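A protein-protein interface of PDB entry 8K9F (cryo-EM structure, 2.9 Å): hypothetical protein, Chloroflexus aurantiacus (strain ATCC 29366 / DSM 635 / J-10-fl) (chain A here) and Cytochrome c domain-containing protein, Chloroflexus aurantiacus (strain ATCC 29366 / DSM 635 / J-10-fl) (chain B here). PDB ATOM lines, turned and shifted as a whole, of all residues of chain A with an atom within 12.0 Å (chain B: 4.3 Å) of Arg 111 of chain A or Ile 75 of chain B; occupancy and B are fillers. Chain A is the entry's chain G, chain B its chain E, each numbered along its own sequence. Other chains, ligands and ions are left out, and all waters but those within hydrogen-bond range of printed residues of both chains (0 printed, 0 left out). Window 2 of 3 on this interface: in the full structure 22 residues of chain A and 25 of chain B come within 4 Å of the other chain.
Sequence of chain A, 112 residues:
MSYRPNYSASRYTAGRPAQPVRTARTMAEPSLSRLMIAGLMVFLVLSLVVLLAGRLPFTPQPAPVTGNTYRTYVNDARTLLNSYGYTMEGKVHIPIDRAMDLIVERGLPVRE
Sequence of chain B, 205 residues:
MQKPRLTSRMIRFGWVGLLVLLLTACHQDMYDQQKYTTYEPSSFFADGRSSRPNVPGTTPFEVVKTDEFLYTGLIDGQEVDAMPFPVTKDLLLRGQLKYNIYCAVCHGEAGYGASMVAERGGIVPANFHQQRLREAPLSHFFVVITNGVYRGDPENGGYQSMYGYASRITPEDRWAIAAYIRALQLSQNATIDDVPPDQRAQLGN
The backbone NH (N) of Met 83 of chain B lies within hydrogen-bond range of the backbone carbonyl oxygen (O) of Pro 109 of chain A (2.8 Å).
The backbone NH of Arg 111 of chain A sits at hydrogen-bond distance from the backbone carbonyl oxygen of Met 83 of chain B, at 2.5 Å.
CA of Ala 82 of chain B touches O of Pro 109 of chain A, 3.3 Å away.
Val 110 of chain A touches Met 83 of chain B (CA to O, 3.3 Å).
Phe 69 of chain B touches Arg 111 of chain A (CB to NH1, 3.8 Å).
CD1 of Ile 75 of chain B touches NH2 of Arg 111 of chain A, 3.7 Å away.
Arg 111 of chain A touches Ala 82 of chain B (N to CB, 3.6 Å).
Printed residues of chain B that touch a printed residue of chain A: Phe 69, Ile 75, Ala 82 and Met 83.
Of the 6 printed residues of chain A, 3 touch a printed residue of chain B.
Printed residues of chain A that touch a printed residue of chain B: Pro 109, Val 110 and Arg 111.
Among the printed residues, 7 pairs touch across the chains.
Among the printed residues, no Asp or Glu carboxylate lies within 4 Å of a Lys or Arg side-chain nitrogen of the other chain.
The side-chain carboxylate (OD1) of Asp 67 of chain B is in hydrogen-bond range of the backbone NH (N) of Phe 69 of chain B (3.0 Å).
Leu 108 of chain A touches none of the printed residues of chain B.
Of the printed residues of chain B, Pro 109 of chain A touches Ala 82 (3.3 Å) and Met 83 (2.8 Å).
Of the printed residues of chain B, Val 110 of chain A touches Met 83.
Of chain B, only Phe 69, Ile 75, Ala 82 and Met 83 come within 4 Å of Arg 111 of chain A.
Asp 67 of chain B touches none of the printed residues of chain A.
No residue of chain A comes within 4 Å of Asp 76 of chain B.
No residue of chain A comes within 4 Å of Gly 77 of chain B.
Val 80 of chain B touches none of the printed residues of chain A.
Of chain A, only Pro 109 and Arg 111 come within 4 Å of Ala 82 of chain B.
Of the printed residues of chain A, Met 83 of chain B touches Pro 109 (2.8 Å), Val 110 (3.3 Å) and Arg 111 (2.5 Å).
The nearest printed residue of chain B that does not touch Pro 109 of chain A is Phe 69 of chain B (6.3 Å).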
ATOM      1  N   ARG A 106      15.381   0.824 -19.939  1.00  0.00           N
ATOM      2  CA  ARG A 106      14.428   0.209 -20.858  1.00  0.00           C
ATOM      3  C   ARG A 106      13.216  -0.343 -20.126  1.00  0.00           C
ATOM      4  O   ARG A 106      12.254  -0.764 -20.775  1.00  0.00           O
ATOM      5  CB  ARG A 106      15.056  -0.906 -21.705  1.00  0.00           C
ATOM      6  CG  ARG A 106      15.871  -1.941 -20.967  1.00  0.00           C
ATOM      7  CD  ARG A 106      16.819  -2.658 -21.914  1.00  0.00           C
ATOM      8  NE  ARG A 106      17.938  -1.818 -22.325  1.00  0.00           N
ATOM      9  CZ  ARG A 106      18.304  -1.634 -23.585  1.00  0.00           C
ATOM     10  NH1 ARG A 106      17.656  -2.210 -24.584  1.00  0.00           N
ATOM     11  NH2 ARG A 106      19.347  -0.852 -23.851  1.00  0.00           N
ATOM     12  N   GLY A 107      13.250  -0.363 -18.800  1.00  0.00           N
ATOM     13  CA  GLY A 107      12.075  -0.590 -17.991  1.00  0.00           C
ATOM     14  C   GLY A 107      11.653  -2.047 -17.940  1.00  0.00           C
ATOM     15  O   GLY A 107      11.963  -2.858 -18.812  1.00  0.00           O
ATOM     16  N   LEU A 108      10.946  -2.379 -16.877  1.00  0.00           N
ATOM     17  CA  LEU A 108      10.177  -3.603 -16.927  1.00  0.00           C
ATOM     18  C   LEU A 108       8.761  -3.272 -17.382  1.00  0.00           C
ATOM     19  O   LEU A 108       8.311  -2.132 -17.213  1.00  0.00           O
ATOM     20  CB  LEU A 108      10.128  -4.323 -15.571  1.00  0.00           C
ATOM     21  CG  LEU A 108      11.257  -5.311 -15.253  1.00  0.00           C
ATOM     22  CD1 LEU A 108      11.462  -6.267 -16.410  1.00  0.00           C
ATOM     23  CD2 LEU A 108      12.554  -4.630 -14.905  1.00  0.00           C
ATOM     24  N   PRO A 109       8.069  -4.211 -18.030  1.00  0.00           N
ATOM     25  CA  PRO A 109       6.661  -3.984 -18.368  1.00  0.00           C
ATOM     26  C   PRO A 109       5.812  -3.799 -17.121  1.00  0.00           C
ATOM     27  O   PRO A 109       6.056  -4.413 -16.082  1.00  0.00           O
ATOM     28  CB  PRO A 109       6.272  -5.253 -19.133  1.00  0.00           C
ATOM     29  CG  PRO A 109       7.546  -5.728 -19.723  1.00  0.00           C
ATOM     30  CD  PRO A 109       8.612  -5.394 -18.720  1.00  0.00           C
ATOM     31  N   VAL A 110       4.826  -2.914 -17.228  1.00  0.00           N
ATOM     32  CA  VAL A 110       3.921  -2.602 -16.132  1.00  0.00           C
ATOM     33  C   VAL A 110       2.534  -3.074 -16.536  1.00  0.00           C
ATOM     34  O   VAL A 110       2.027  -2.684 -17.596  1.00  0.00           O
ATOM     35  CB  VAL A 110       3.923  -1.101 -15.803  1.00  0.00           C
ATOM     36  CG1 VAL A 110       2.925  -0.794 -14.695  1.00  0.00           C
ATOM     37  CG2 VAL A 110       5.322  -0.642 -15.430  1.00  0.00           C
ATOM     38  N   ARG A 111       1.941  -3.927 -15.699  1.00  0.00           N
ATOM     39  CA  ARG A 111       0.579  -4.461 -15.846  1.00  0.00           C
ATOM     40  C   ARG A 111       0.290  -5.133 -17.185  1.00  0.00           C
ATOM     41  O   ARG A 111      -0.797  -4.982 -17.737  1.00  0.00           O
ATOM     42  CB  ARG A 111      -0.455  -3.360 -15.612  1.00  0.00           C
ATOM     43  CG  ARG A 111      -0.745  -3.092 -14.153  1.00  0.00           C
ATOM     44  CD  ARG A 111      -2.240  -3.025 -13.934  1.00  0.00           C
ATOM     45  NE  ARG A 111      -2.930  -4.025 -14.743  1.00  0.00           N
ATOM     46  CZ  ARG A 111      -3.218  -5.254 -14.333  1.00  0.00           C
ATOM     47  NH1 ARG A 111      -2.928  -5.659 -13.108  1.00  0.00           N
ATOM     48  NH2 ARG A 111      -3.804  -6.098 -15.174  1.00  0.00           N
ATOM     49  N   ASP B  67      -6.240  -6.149  -5.605  1.00  0.00           N
ATOM     50  CA  ASP B  67      -5.550  -6.264  -6.884  1.00  0.00           C
ATOM     51  C   ASP B  67      -4.790  -7.581  -6.851  1.00  0.00           C
ATOM     52  O   ASP B  67      -3.835  -7.729  -6.080  1.00  0.00           O
ATOM     53  CB  ASP B  67      -4.638  -5.044  -7.123  1.00  0.00           C
ATOM     54  CG  ASP B  67      -3.692  -5.182  -8.339  1.00  0.00           C
ATOM     55  OD1 ASP B  67      -2.782  -6.043  -8.387  1.00  0.00           O
ATOM     56  OD2 ASP B  67      -3.879  -4.393  -9.287  1.00  0.00           O
ATOM     57  N   PHE B  69      -2.815  -9.020  -9.043  1.00  0.00           N
ATOM     58  CA  PHE B  69      -1.473  -9.105  -9.609  1.00  0.00           C
ATOM     59  C   PHE B  69      -0.399  -8.700  -8.607  1.00  0.00           C
ATOM     60  O   PHE B  69       0.748  -9.144  -8.720  1.00  0.00           O
ATOM     61  CB  PHE B  69      -1.385  -8.252 -10.871  1.00  0.00           C
ATOM     62  CG  PHE B  69      -0.162  -8.512 -11.689  1.00  0.00           C
ATOM     63  CD1 PHE B  69       0.313  -9.801 -11.856  1.00  0.00           C
ATOM     64  CD2 PHE B  69       0.538  -7.465 -12.256  1.00  0.00           C
ATOM     65  CE1 PHE B  69       1.449 -10.042 -12.596  1.00  0.00           C
ATOM     66  CE2 PHE B  69       1.669  -7.703 -13.006  1.00  0.00           C
ATOM     67  CZ  PHE B  69       2.125  -8.994 -13.174  1.00  0.00           C
ATOM     68  N   GLY B  73       0.927 -14.038  -8.751  1.00  0.00           N
ATOM     69  CA  GLY B  73       1.478 -13.791 -10.068  1.00  0.00           C
ATOM     70  C   GLY B  73       0.508 -13.950 -11.216  1.00  0.00           C
ATOM     71  O   GLY B  73       0.892 -13.746 -12.369  1.00  0.00           O
ATOM     72  N   LEU B  74      -0.742 -14.300 -10.935  1.00  0.00           N
ATOM     73  CA  LEU B  74      -1.691 -14.714 -11.957  1.00  0.00           C
ATOM     74  C   LEU B  74      -2.852 -13.732 -11.996  1.00  0.00           C
ATOM     75  O   LEU B  74      -3.520 -13.517 -10.979  1.00  0.00           O
ATOM     76  CB  LEU B  74      -2.196 -16.131 -11.674  1.00  0.00           C
ATOM     77  CG  LEU B  74      -1.433 -17.413 -12.057  1.00  0.00           C
ATOM     78  CD1 LEU B  74       0.059 -17.410 -11.780  1.00  0.00           C
ATOM     79  CD2 LEU B  74      -2.088 -18.605 -11.373  1.00  0.00           C
ATOM     80  N   ILE B  75      -3.097 -13.143 -13.162  1.00  0.00           N
ATOM     81  CA  ILE B  75      -4.292 -12.334 -13.392  1.00  0.00           C
ATOM     82  C   ILE B  75      -5.386 -13.144 -14.073  1.00  0.00           C
ATOM     83  O   ILE B  75      -6.484 -13.293 -13.538  1.00  0.00           O
ATOM     84  CB  ILE B  75      -3.953 -11.066 -14.205  1.00  0.00           C
ATOM     85  CG1 ILE B  75      -2.560 -10.557 -13.859  1.00  0.00           C
ATOM     86  CG2 ILE B  75      -4.985  -9.984 -13.949  1.00  0.00           C
ATOM     87  CD1 ILE B  75      -2.148  -9.336 -14.662  1.00  0.00           C
ATOM     88  N   ASP B  76      -5.103 -13.673 -15.262  1.00  0.00           N
ATOM     89  CA  ASP B  76      -6.022 -14.564 -15.952  1.00  0.00           C
ATOM     90  C   ASP B  76      -5.757 -16.028 -15.631  1.00  0.00           C
ATOM     91  O   ASP B  76      -6.417 -16.907 -16.196  1.00  0.00           O
ATOM     92  CB  ASP B  76      -5.965 -14.336 -17.469  1.00  0.00           C
ATOM     93  CG  ASP B  76      -4.543 -14.190 -18.003  1.00  0.00           C
ATOM     94  OD1 ASP B  76      -3.631 -14.925 -17.562  1.00  0.00           O
ATOM     95  OD2 ASP B  76      -4.340 -13.332 -18.886  1.00  0.00           O
ATOM     96  N   GLY B  77      -4.808 -16.305 -14.738  1.00  0.00           N
ATOM     97  CA  GLY B  77      -4.419 -17.657 -14.404  1.00  0.00           C
ATOM     98  C   GLY B  77      -3.114 -18.121 -15.012  1.00  0.00           C
ATOM     99  O   GLY B  77      -2.642 -19.208 -14.661  1.00  0.00           O
ATOM    100  N   VAL B  80       2.492 -13.546 -16.831  1.00  0.00           N
ATOM    101  CA  VAL B  80       2.116 -12.208 -17.271  1.00  0.00           C
ATOM    102  C   VAL B  80       3.245 -11.455 -17.977  1.00  0.00           C
ATOM    103  O   VAL B  80       2.968 -10.780 -18.984  1.00  0.00           O
ATOM    104  CB  VAL B  80       1.574 -11.377 -16.086  1.00  0.00           C
ATOM    105  CG1 VAL B  80       0.987 -10.057 -16.552  1.00  0.00           C
ATOM    106  CG2 VAL B  80       0.522 -12.163 -15.328  1.00  0.00           C
ATOM    107  N   ALA B  82       5.035  -8.890 -16.688  1.00  0.00           N
ATOM    108  CA  ALA B  82       4.807  -7.487 -16.369  1.00  0.00           C
ATOM    109  C   ALA B  82       4.888  -7.326 -14.856  1.00  0.00           C
ATOM    110  O   ALA B  82       5.135  -8.285 -14.124  1.00  0.00           O
ATOM    111  CB  ALA B  82       3.459  -7.000 -16.914  1.00  0.00           C
ATOM    112  N   MET B  83       4.681  -6.098 -14.393  1.00  0.00           N
ATOM    113  CA  MET B  83       4.757  -5.746 -12.985  1.00  0.00           C
ATOM    114  C   MET B  83       3.576  -4.876 -12.580  1.00  0.00           C
ATOM    115  O   MET B  83       2.937  -4.258 -13.435  1.00  0.00           O
ATOM    116  CB  MET B  83       6.064  -5.008 -12.659  1.00  0.00           C
ATOM    117  CG  MET B  83       7.314  -5.819 -12.857  1.00  0.00           C
ATOM    118  SD  MET B  83       7.893  -6.307 -11.225  1.00  0.00           S
ATOM    119  CE  MET B  83       9.212  -5.149 -10.988  1.00  0.00           C
